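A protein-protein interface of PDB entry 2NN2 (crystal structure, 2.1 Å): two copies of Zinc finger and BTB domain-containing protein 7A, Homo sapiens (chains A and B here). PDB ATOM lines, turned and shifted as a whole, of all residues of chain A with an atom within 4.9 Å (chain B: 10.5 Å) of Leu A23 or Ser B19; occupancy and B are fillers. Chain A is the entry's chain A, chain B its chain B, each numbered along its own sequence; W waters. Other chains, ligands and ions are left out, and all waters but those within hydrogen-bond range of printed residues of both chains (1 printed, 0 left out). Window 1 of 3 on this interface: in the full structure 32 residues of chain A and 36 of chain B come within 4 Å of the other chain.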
ATOM      1  N   SER A  19       1.458  -7.344   6.987  1.00  0.00           N
ATOM      2  CA  SER A  19       0.339  -6.405   7.171  1.00  0.00           C
ATOM      3  C   SER A  19       0.612  -5.341   8.273  1.00  0.00           C
ATOM      4  O   SER A  19       0.277  -4.188   8.098  1.00  0.00           O
ATOM      5  CB  SER A  19      -1.013  -7.153   7.346  1.00  0.00           C
ATOM      6  OG  SER A  19      -1.071  -7.839   8.586  1.00  0.00           O
ATOM      7  N   SER A  20       1.219  -5.746   9.388  1.00  0.00           N
ATOM      8  CA  SER A  20       1.758  -4.823  10.385  1.00  0.00           C
ATOM      9  C   SER A  20       2.763  -3.850   9.829  1.00  0.00           C
ATOM     10  O   SER A  20       2.665  -2.659  10.098  1.00  0.00           O
ATOM     11  CB  SER A  20       2.384  -5.583  11.572  1.00  0.00           C
ATOM     12  OG  SER A  20       1.332  -6.183  12.309  1.00  0.00           O
ATOM     13  N   ASP A  21       3.740  -4.339   9.053  1.00  0.00           N
ATOM     14  CA  ASP A  21       4.690  -3.426   8.389  1.00  0.00           C
ATOM     15  C   ASP A  21       4.021  -2.458   7.385  1.00  0.00           C
ATOM     16  O   ASP A  21       4.403  -1.284   7.335  1.00  0.00           O
ATOM     17  CB  ASP A  21       5.842  -4.188   7.691  1.00  0.00           C
ATOM     18  CG  ASP A  21       6.625  -5.096   8.636  1.00  0.00           C
ATOM     19  OD1 ASP A  21       6.510  -4.949   9.889  1.00  0.00           O
ATOM     20  OD2 ASP A  21       7.374  -5.995   8.131  1.00  0.00           O
ATOM     21  N   ILE A  22       3.044  -2.925   6.573  1.00  0.00           N
ATOM     22  CA  ILE A  22       2.340  -2.024   5.681  1.00  0.00           C
ATOM     23  C   ILE A  22       1.598  -0.909   6.518  1.00  0.00           C
ATOM     24  O   ILE A  22       1.628   0.287   6.195  1.00  0.00           O
ATOM     25  CB  ILE A  22       1.296  -2.801   4.807  1.00  0.00           C
ATOM     26  CG1 ILE A  22       2.004  -3.672   3.751  1.00  0.00           C
ATOM     27  CG2 ILE A  22       0.353  -1.842   4.056  1.00  0.00           C
ATOM     28  CD1 ILE A  22       2.823  -2.885   2.755  1.00  0.00           C
ATOM     29  N   LEU A  23       0.935  -1.326   7.589  1.00  0.00           N
ATOM     30  CA  LEU A  23       0.191  -0.334   8.448  1.00  0.00           C
ATOM     31  C   LEU A  23       1.160   0.633   9.124  1.00  0.00           C
ATOM     32  O   LEU A  23       0.908   1.833   9.204  1.00  0.00           O
ATOM     33  CB  LEU A  23      -0.679  -1.059   9.491  1.00  0.00           C
ATOM     34  CG  LEU A  23      -1.842  -0.276  10.150  1.00  0.00           C
ATOM     35  CD1 LEU A  23      -2.803   0.347   9.124  1.00  0.00           C
ATOM     36  CD2 LEU A  23      -2.622  -1.210  11.088  1.00  0.00           C
ATOM     37  N   SER A  24       2.275   0.110   9.617  1.00  0.00           N
ATOM     38  CA  SER A  24       3.321   0.969  10.161  1.00  0.00           C
ATOM     39  C   SER A  24       3.833   2.021   9.164  1.00  0.00           C
ATOM     40  O   SER A  24       4.083   3.172   9.543  1.00  0.00           O
ATOM     41  CB  SER A  24       4.461   0.117  10.698  1.00  0.00           C
ATOM     42  OG  SER A  24       5.384   0.941  11.389  1.00  0.00           O
ATOM     43  N   GLY A  25       4.001   1.622   7.895  1.00  0.00           N
ATOM     44  CA  GLY A  25       4.343   2.563   6.821  1.00  0.00           C
ATOM     45  C   GLY A  25       3.282   3.625   6.534  1.00  0.00           C
ATOM     46  O   GLY A  25       3.618   4.806   6.328  1.00  0.00           O
ATOM     47  N   LEU A  26       2.013   3.228   6.496  1.00  0.00           N
ATOM     48  CA  LEU A  26       0.909   4.171   6.323  1.00  0.00           C
ATOM     49  C   LEU A  26       0.805   5.146   7.534  1.00  0.00           C
ATOM     50  O   LEU A  26       0.514   6.335   7.363  1.00  0.00           O
ATOM     51  CB  LEU A  26      -0.413   3.410   6.110  1.00  0.00           C
ATOM     52  CG  LEU A  26      -0.526   2.470   4.901  1.00  0.00           C
ATOM     53  CD1 LEU A  26      -1.841   1.633   4.836  1.00  0.00           C
ATOM     54  CD2 LEU A  26      -0.388   3.249   3.626  1.00  0.00           C
ATOM     55  N   ASN A  27       1.070   4.637   8.735  1.00  0.00           N
ATOM     56  CA  ASN A  27       1.054   5.478   9.945  1.00  0.00           C
ATOM     57  C   ASN A  27       2.188   6.522   9.921  1.00  0.00           C
ATOM     58  O   ASN A  27       1.937   7.680  10.183  1.00  0.00           O
ATOM     59  CB  ASN A  27       1.113   4.619  11.226  1.00  0.00           C
ATOM     60  CG  ASN A  27       0.916   5.453  12.503  1.00  0.00           C
ATOM     61  OD1 ASN A  27       0.051   6.325  12.559  1.00  0.00           O
ATOM     62  ND2 ASN A  27       1.733   5.184  13.524  1.00  0.00           N
ATOM     63  N   ALA A  94      -7.186   3.086  13.763  1.00  0.00           N
ATOM     64  CA  ALA A  94      -7.173   2.688  12.356  1.00  0.00           C
ATOM     65  C   ALA A  94      -5.762   2.519  11.861  1.00  0.00           C
ATOM     66  O   ALA A  94      -5.499   1.617  11.085  1.00  0.00           O
ATOM     67  CB  ALA A  94      -7.881   3.705  11.503  1.00  0.00           C
ATOM     68  N   TYR A  95      -4.844   3.372  12.308  1.00  0.00           N
ATOM     69  CA  TYR A  95      -3.451   3.330  11.848  1.00  0.00           C
ATOM     70  C   TYR A  95      -2.495   2.525  12.731  1.00  0.00           C
ATOM     71  O   TYR A  95      -1.335   2.294  12.349  1.00  0.00           O
ATOM     72  CB  TYR A  95      -2.903   4.736  11.699  1.00  0.00           C
ATOM     73  CG  TYR A  95      -3.354   5.419  10.413  1.00  0.00           C
ATOM     74  CD1 TYR A  95      -4.542   6.136  10.364  1.00  0.00           C
ATOM     75  CD2 TYR A  95      -2.574   5.342   9.246  1.00  0.00           C
ATOM     76  CE1 TYR A  95      -4.950   6.760   9.181  1.00  0.00           C
ATOM     77  CE2 TYR A  95      -2.952   5.975   8.077  1.00  0.00           C
ATOM     78  CZ  TYR A  95      -4.140   6.685   8.043  1.00  0.00           C
ATOM     79  OH  TYR A  95      -4.539   7.283   6.857  1.00  0.00           O
ATOM     80  N   THR A  96      -2.905   2.155  13.943  1.00  0.00           N
ATOM     81  CA  THR A  96      -1.939   1.442  14.786  1.00  0.00           C
ATOM     82  C   THR A  96      -2.418   0.114  15.339  1.00  0.00           C
ATOM     83  O   THR A  96      -1.606  -0.586  15.946  1.00  0.00           O
ATOM     84  CB  THR A  96      -1.421   2.260  16.007  1.00  0.00           C
ATOM     85  OG1 THR A  96      -2.439   2.263  16.998  1.00  0.00           O
ATOM     86  CG2 THR A  96      -1.040   3.691  15.671  1.00  0.00           C
ATOM     87  N   ALA A  97      -3.701  -0.210  15.176  1.00  0.00           N
ATOM     88  CA  ALA A  97      -4.321  -1.386  15.787  1.00  0.00           C
ATOM     89  C   ALA A  97      -4.549  -1.364  17.339  1.00  0.00           C
ATOM     90  O   ALA A  97      -4.853  -2.399  17.926  1.00  0.00           O
ATOM     91  CB  ALA A  97      -3.556  -2.691  15.386  1.00  0.00           C
ATOM     92  N   PRO B  14      -5.105  -3.627  22.483  1.00  0.00           N
ATOM     93  CA  PRO B  14      -4.654  -4.152  21.155  1.00  0.00           C
ATOM     94  C   PRO B  14      -5.703  -5.003  20.433  1.00  0.00           C
ATOM     95  O   PRO B  14      -6.422  -5.754  21.068  1.00  0.00           O
ATOM     96  CB  PRO B  14      -3.427  -5.005  21.515  1.00  0.00           C
ATOM     97  CG  PRO B  14      -3.730  -5.498  22.947  1.00  0.00           C
ATOM     98  CD  PRO B  14      -4.503  -4.372  23.614  1.00  0.00           C
ATOM     99  N   PHE B  15      -5.800  -4.835  19.105  1.00  0.00           N
ATOM    100  CA  PHE B  15      -6.641  -5.649  18.224  1.00  0.00           C
ATOM    101  C   PHE B  15      -5.694  -6.404  17.264  1.00  0.00           C
ATOM    102  O   PHE B  15      -5.284  -5.863  16.213  1.00  0.00           O
ATOM    103  CB  PHE B  15      -7.630  -4.781  17.414  1.00  0.00           C
ATOM    104  CG  PHE B  15      -8.681  -4.101  18.264  1.00  0.00           C
ATOM    105  CD1 PHE B  15      -8.336  -3.017  19.084  1.00  0.00           C
ATOM    106  CD2 PHE B  15      -9.998  -4.563  18.273  1.00  0.00           C
ATOM    107  CE1 PHE B  15      -9.309  -2.380  19.900  1.00  0.00           C
ATOM    108  CE2 PHE B  15     -10.973  -3.936  19.102  1.00  0.00           C
ATOM    109  CZ  PHE B  15     -10.625  -2.857  19.896  1.00  0.00           C
ATOM    110  N   PRO B  16      -5.312  -7.636  17.644  1.00  0.00           N
ATOM    111  CA  PRO B  16      -4.242  -8.331  16.913  1.00  0.00           C
ATOM    112  C   PRO B  16      -4.492  -8.622  15.429  1.00  0.00           C
ATOM    113  O   PRO B  16      -3.515  -8.747  14.687  1.00  0.00           O
ATOM    114  CB  PRO B  16      -4.028  -9.619  17.717  1.00  0.00           C
ATOM    115  CG  PRO B  16      -5.312  -9.817  18.466  1.00  0.00           C
ATOM    116  CD  PRO B  16      -5.813  -8.421  18.784  1.00  0.00           C
ATOM    117  N   ASP B  17      -5.750  -8.715  14.981  1.00  0.00           N
ATOM    118  CA  ASP B  17      -6.006  -8.954  13.565  1.00  0.00           C
ATOM    119  C   ASP B  17      -6.403  -7.696  12.740  1.00  0.00           C
ATOM    120  O   ASP B  17      -6.648  -7.767  11.540  1.00  0.00           O
ATOM    121  CB  ASP B  17      -7.000 -10.111  13.383  1.00  0.00           C
ATOM    122  CG  ASP B  17      -6.441 -11.480  13.950  1.00  0.00           C
ATOM    123  OD1 ASP B  17      -5.291 -11.861  13.610  1.00  0.00           O
ATOM    124  OD2 ASP B  17      -7.169 -12.168  14.732  1.00  0.00           O
ATOM    125  N   HIS B  18      -6.409  -6.541  13.369  1.00  0.00           N
ATOM    126  CA  HIS B  18      -6.812  -5.293  12.676  1.00  0.00           C
ATOM    127  C   HIS B  18      -5.968  -5.016  11.401  1.00  0.00           C
ATOM    128  O   HIS B  18      -6.509  -4.716  10.359  1.00  0.00           O
ATOM    129  CB  HIS B  18      -6.778  -4.099  13.635  1.00  0.00           C
ATOM    130  CG  HIS B  18      -7.000  -2.779  12.954  1.00  0.00           C
ATOM    131  ND1 HIS B  18      -8.230  -2.398  12.456  1.00  0.00           N
ATOM    132  CD2 HIS B  18      -6.136  -1.792  12.619  1.00  0.00           C
ATOM    133  CE1 HIS B  18      -8.127  -1.201  11.899  1.00  0.00           C
ATOM    134  NE2 HIS B  18      -6.858  -0.820  11.962  1.00  0.00           N
ATOM    135  N   SER B  19      -4.651  -5.115  11.488  1.00  0.00           N
ATOM    136  CA  SER B  19      -3.781  -4.822  10.330  1.00  0.00           C
ATOM    137  C   SER B  19      -4.127  -5.660   9.075  1.00  0.00           C
ATOM    138  O   SER B  19      -4.091  -5.145   7.959  1.00  0.00           O
ATOM    139  CB  SER B  19      -2.284  -4.878  10.711  1.00  0.00           C
ATOM    140  OG  SER B  19      -1.792  -6.199  10.895  1.00  0.00           O
ATOM    141  N   SER B  20      -4.581  -6.904   9.284  1.00  0.00           N
ATOM    142  CA  SER B  20      -5.003  -7.786   8.201  1.00  0.00           C
ATOM    143  C   SER B  20      -6.331  -7.427   7.651  1.00  0.00           C
ATOM    144  O   SER B  20      -6.579  -7.645   6.479  1.00  0.00           O
ATOM    145  CB  SER B  20      -5.029  -9.268   8.672  1.00  0.00           C
ATOM    146  OG  SER B  20      -3.725  -9.539   9.223  1.00  0.00           O
ATOM    147  N   ASP B  21      -7.223  -6.951   8.520  1.00  0.00           N
ATOM    148  CA  ASP B  21      -8.500  -6.330   8.115  1.00  0.00           C
ATOM    149  C   ASP B  21      -8.327  -5.091   7.229  1.00  0.00           C
ATOM    150  O   ASP B  21      -8.996  -4.918   6.229  1.00  0.00           O
ATOM    151  CB  ASP B  21      -9.306  -5.934   9.374  1.00  0.00           C
ATOM    152  CG  ASP B  21      -9.958  -7.141  10.082  1.00  0.00           C
ATOM    153  OD1 ASP B  21     -10.017  -8.283   9.505  1.00  0.00           O
ATOM    154  OD2 ASP B  21     -10.447  -6.919  11.236  1.00  0.00           O
ATOM    155  N   ILE B  22      -7.446  -4.202   7.612  1.00  0.00           N
ATOM    156  CA  ILE B  22      -7.146  -3.019   6.775  1.00  0.00           C
ATOM    157  C   ILE B  22      -6.623  -3.437   5.368  1.00  0.00           C
ATOM    158  O   ILE B  22      -7.124  -3.012   4.329  1.00  0.00           O
ATOM    159  CB  ILE B  22      -6.144  -2.093   7.516  1.00  0.00           C
ATOM    160  CG1 ILE B  22      -6.875  -1.349   8.651  1.00  0.00           C
ATOM    161  CG2 ILE B  22      -5.560  -1.027   6.585  1.00  0.00           C
ATOM    162  CD1 ILE B  22      -8.006  -0.476   8.175  1.00  0.00           C
ATOM    163  N   LEU B  23      -5.651  -4.348   5.352  1.00  0.00           N
ATOM    164  CA  LEU B  23      -5.064  -4.810   4.082  1.00  0.00           C
ATOM    165  C   LEU B  23      -6.129  -5.503   3.218  1.00  0.00           C
ATOM    166  O   LEU B  23      -6.149  -5.349   2.010  1.00  0.00           O
ATOM    167  CB  LEU B  23      -3.860  -5.743   4.376  1.00  0.00           C
ATOM    168  CG  LEU B  23      -2.842  -5.969   3.219  1.00  0.00           C
ATOM    169  CD1 LEU B  23      -2.110  -4.661   2.879  1.00  0.00           C
ATOM    170  CD2 LEU B  23      -1.842  -7.033   3.590  1.00  0.00           C
ATOM    171  N   SER B  24      -7.006  -6.298   3.833  1.00  0.00           N
ATOM    172  CA  SER B  24      -8.108  -6.949   3.112  1.00  0.00           C
ATOM    173  C   SER B  24      -8.992  -5.933   2.446  1.00  0.00           C
ATOM    174  O   SER B  24      -9.470  -6.134   1.336  1.00  0.00           O
ATOM    175  CB  SER B  24      -8.985  -7.770   4.100  1.00  0.00           C
ATOM    176  OG  SER B  24      -9.896  -8.584   3.394  1.00  0.00           O
ATOM    177  N   GLY B  25      -9.268  -4.831   3.136  1.00  0.00           N
ATOM    178  CA  GLY B  25     -10.102  -3.771   2.519  1.00  0.00           C
ATOM    179  C   GLY B  25      -9.343  -3.067   1.387  1.00  0.00           C
ATOM    180  O   GLY B  25      -9.920  -2.761   0.375  1.00  0.00           O
ATOM    181  N   LEU B  26      -8.046  -2.809   1.564  1.00  0.00           N
ATOM    182  CA  LEU B  26      -7.243  -2.198   0.515  1.00  0.00           C
ATOM    183  C   LEU B  26      -7.218  -3.103  -0.725  1.00  0.00           C
ATOM    184  O   LEU B  26      -7.313  -2.619  -1.870  1.00  0.00           O
ATOM    185  CB  LEU B  26      -5.817  -1.829   1.036  1.00  0.00           C
ATOM    186  CG  LEU B  26      -5.768  -0.783   2.149  1.00  0.00           C
ATOM    187  CD1 LEU B  26      -4.327  -0.533   2.742  1.00  0.00           C
ATOM    188  CD2 LEU B  26      -6.298   0.501   1.605  1.00  0.00           C
ATOM    189  N   ASN B  27      -7.138  -4.414  -0.494  1.00  0.00           N
ATOM    190  CA  ASN B  27      -7.090  -5.382  -1.585  1.00  0.00           C
ATOM    191  C   ASN B  27      -8.408  -5.431  -2.345  1.00  0.00           C
ATOM    192  O   ASN B  27      -8.403  -5.512  -3.549  1.00  0.00           O
ATOM    193  CB  ASN B  27      -6.708  -6.774  -1.064  1.00  0.00           C
ATOM    194  CG  ASN B  27      -6.397  -7.779  -2.185  1.00  0.00           C
ATOM    195  OD1 ASN B  27      -5.744  -7.455  -3.185  1.00  0.00           O
ATOM    196  ND2 ASN B  27      -6.850  -9.014  -1.992  1.00  0.00           N
ATOM    197  N   SER B  52       0.319   5.190  -1.757  1.00  0.00           N
ATOM    198  CA  SER B  52       0.632   5.035  -0.348  1.00  0.00           C
ATOM    199  C   SER B  52       0.992   3.606  -0.003  1.00  0.00           C
ATOM    200  O   SER B  52       1.938   3.371   0.760  1.00  0.00           O
ATOM    201  CB  SER B  52      -0.524   5.496   0.560  1.00  0.00           C
ATOM    202  OG  SER B  52      -1.721   4.717   0.325  1.00  0.00           O
ATOM    203  N   VAL B  53       0.207   2.660  -0.480  1.00  0.00           N
ATOM    204  CA  VAL B  53       0.533   1.244  -0.232  1.00  0.00           C
ATOM    205  C   VAL B  53       1.828   0.795  -0.929  1.00  0.00           C
ATOM    206  O   VAL B  53       2.630   0.044  -0.339  1.00  0.00           O
ATOM    207  CB  VAL B  53      -0.641   0.298  -0.625  1.00  0.00           C
ATOM    208  CG1 VAL B  53      -0.275  -1.171  -0.363  1.00  0.00           C
ATOM    209  CG2 VAL B  53      -1.941   0.695   0.153  1.00  0.00           C
ATOM    210  N   LEU B  54       2.021   1.198  -2.192  1.00  0.00           N
ATOM    211  CA  LEU B  54       3.269   0.859  -2.901  1.00  0.00           C
ATOM    212  C   LEU B  54       4.492   1.446  -2.196  1.00  0.00           C
ATOM    213  O   LEU B  54       5.469   0.745  -1.997  1.00  0.00           O
ATOM    214  CB  LEU B  54       3.247   1.358  -4.365  1.00  0.00           C
ATOM    215  CG  LEU B  54       2.261   0.653  -5.334  1.00  0.00           C
ATOM    216  CD1 LEU B  54       2.328   1.281  -6.731  1.00  0.00           C
ATOM    217  CD2 LEU B  54       2.566  -0.809  -5.456  1.00  0.00           C
ATOM    218  N   ALA B  55       4.435   2.710  -1.813  1.00  0.00           N
ATOM    219  CA  ALA B  55       5.536   3.357  -1.003  1.00  0.00           C
ATOM    220  C   ALA B  55       5.845   2.688   0.352  1.00  0.00           C
ATOM    221  O   ALA B  55       7.005   2.652   0.793  1.00  0.00           O
ATOM    222  CB  ALA B  55       5.179   4.825  -0.761  1.00  0.00           C
ATOM    223  N   ALA B  56       4.810   2.203   1.037  1.00  0.00           N
ATOM    224  CA  ALA B  56       4.939   1.463   2.309  1.00  0.00           C
ATOM    225  C   ALA B  56       5.606   0.088   2.074  1.00  0.00           C
ATOM    226  O   ALA B  56       6.211  -0.501   2.969  1.00  0.00           O
ATOM    227  CB  ALA B  56       3.564   1.283   2.933  1.00  0.00           C
ATOM    228  N   CYS B  57       5.497  -0.404   0.857  1.00  0.00           N
ATOM    229  CA  CYS B  57       5.953  -1.725   0.520  1.00  0.00           C
ATOM    230  C   CYS B  57       7.328  -1.714  -0.185  1.00  0.00           C
ATOM    231  O   CYS B  57       8.126  -2.645  -0.001  1.00  0.00           O
ATOM    232  CB  CYS B  57       4.873  -2.403  -0.374  1.00  0.00           C
ATOM    233  SG  CYS B  57       5.331  -4.071  -0.838  1.00  0.00           S
ATOM    234  N   ALA B  94       1.962  -7.550  -1.966  1.00  0.00           N
ATOM    235  CA  ALA B  94       1.797  -6.260  -1.239  1.00  0.00           C
ATOM    236  C   ALA B  94       0.444  -6.127  -0.546  1.00  0.00           C
ATOM    237  O   ALA B  94       0.371  -5.608   0.564  1.00  0.00           O
ATOM    238  CB  ALA B  94       1.982  -5.071  -2.176  1.00  0.00           C
ATOM    239  N   TYR B  95      -0.602  -6.586  -1.239  1.00  0.00           N
ATOM    240  CA  TYR B  95      -1.975  -6.546  -0.788  1.00  0.00           C
ATOM    241  C   TYR B  95      -2.471  -7.780  -0.037  1.00  0.00           C
ATOM    242  O   TYR B  95      -3.527  -7.695   0.569  1.00  0.00           O
ATOM    243  CB  TYR B  95      -2.893  -6.283  -1.998  1.00  0.00           C
ATOM    244  CG  TYR B  95      -2.843  -4.839  -2.483  1.00  0.00           C
ATOM    245  CD1 TYR B  95      -3.632  -3.872  -1.888  1.00  0.00           C
ATOM    246  CD2 TYR B  95      -2.013  -4.455  -3.544  1.00  0.00           C
ATOM    247  CE1 TYR B  95      -3.616  -2.540  -2.311  1.00  0.00           C
ATOM    248  CE2 TYR B  95      -1.976  -3.100  -3.994  1.00  0.00           C
ATOM    249  CZ  TYR B  95      -2.790  -2.160  -3.369  1.00  0.00           C
ATOM    250  OH  TYR B  95      -2.787  -0.850  -3.775  1.00  0.00           O
ATOM    251  N   THR B  96      -1.756  -8.913  -0.089  1.00  0.00           N
ATOM    252  CA  THR B  96      -2.163 -10.115   0.646  1.00  0.00           C
ATOM    253  C   THR B  96      -1.227 -10.704   1.702  1.00  0.00           C
ATOM    254  O   THR B  96      -1.667 -11.520   2.525  1.00  0.00           O
ATOM    255  CB  THR B  96      -2.539 -11.284  -0.272  1.00  0.00           C
ATOM    256  OG1 THR B  96      -1.369 -11.722  -0.976  1.00  0.00           O
ATOM    257  CG2 THR B  96      -3.622 -10.858  -1.273  1.00  0.00           C
ATOM    258  N   ALA B  97       0.038 -10.301   1.727  1.00  0.00           N
ATOM    259  CA  ALA B  97       1.010 -10.925   2.620  1.00  0.00           C
ATOM    260  C   ALA B  97       1.482 -12.352   2.235  1.00  0.00           C
ATOM    261  O   ALA B  97       2.216 -12.948   3.013  1.00  0.00           O
ATOM    262  CB  ALA B  97       0.548 -10.892   4.075  1.00  0.00           C
HETATM  263  O   HOH W   1      -1.495 -10.843   6.953  1.00  0.00           O
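OG of Ser A19 is in hydrogen-bond range of OG of Ser B19 (2.9 Å). OG of Ser B20 is in hydrogen-bond range of OG of Ser A19 (3.2 Å). The backbone NH of Ser A20 sits at hydrogen-bond distance from the side-chain hydroxyl of Ser B19 (3.4 Å). NE2 of His B18 sits at hydrogen-bond distance from O of Ala A94, at 2.9 Å. The backbone carbonyl oxygen of Ala A97 lies within hydrogen-bond range of the backbone NH of Phe B15.
Ser A19 touches Leu B23. Ile A22 touches Leu B23. CB of Ala B56 touches O of Ile A22 (3.9 Å). CD1 of Ile A22 touches CB of Cys B57, at 3.8 Å. Leu A23 touches His B18 (CD2 to CD2, 3.9 Å). Leu A23 touches Ser B19. Ile B22 touches Leu A23 (CG2 to CD1, 3.99 Å). Leu A26 touches Leu B26. Leu A26 touches Ser B52. Pro B14 touches Ala A97 (CA to O, 3.7 Å).
Ser A19 touches just these residues of chain B: Ser B19, Ser B20 and Leu B23. Of the printed residues of chain B, Leu A23 touches His B18, Ser B19 and Ile B22. Of chain B, only Leu B26 and Ser B52 come within 4 Å of Leu A26. No residue of chain B comes within 4 Å of Asn A27. Printed residues of chain A within 4 Å of Pro B14: Ala A97 (3.7 Å). Pro B16 touches none of the printed residues of chain A. Printed residues of chain A within 4 Å of His B18: Leu A23 (3.9 Å), Ala A94 (2.9 Å) and Ala A97 (3.7 Å). Printed residues of chain A within 4 Å of Ile B22: Leu A23. Gly B25 touches none of the printed residues of chain A. Of the printed residues of chain A, Leu B26 touches Leu A26. Of the printed residues of chain A, Cys B57 touches Ile A22. The nearest printed residue of chain B that does not touch Leu A23 is Ala B56 (5.9 Å). The nearest residue of chain A that does not touch Ser B19 is Ala A97 (4.7 Å). The nearest printed residue of chain A that does not touch Ile B22 is Ala A94 (4.1 Å).
Of the 13 printed residues of chain A, 7 touch a printed residue of chain B. Printed residues of chain B that touch a printed residue of chain A: Pro B14, Phe B15, His B18, Ser B19, Ser B20, Ile B22, Leu B23, Leu B26, Ser B52, Ala B56 and Cys B57.
Ser A19 touches its own counterpart, Ser B19. Ser A19 touches Ser B20, and with the chains exchanged Ser A20 touches Ser B19. Ser A19 touches Leu B23, and with the chains exchanged Leu A23 touches Ser B19. Ile A22 touches Leu B23, and with the chains exchanged Leu A23 touches Ile B22. Positions printed for both chains: 19, 20, 21, 22, 23, 24, 25, 26, 27, 94, 95, 96 and 97. Of the 16 pairs that touch across the chains among the printed residues, 8 have their exchanged pair printed and touching as well.
Water W1 bridges the side-chain hydroxyl of Ser B20 and the side-chain hydroxyl of Ser A19.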
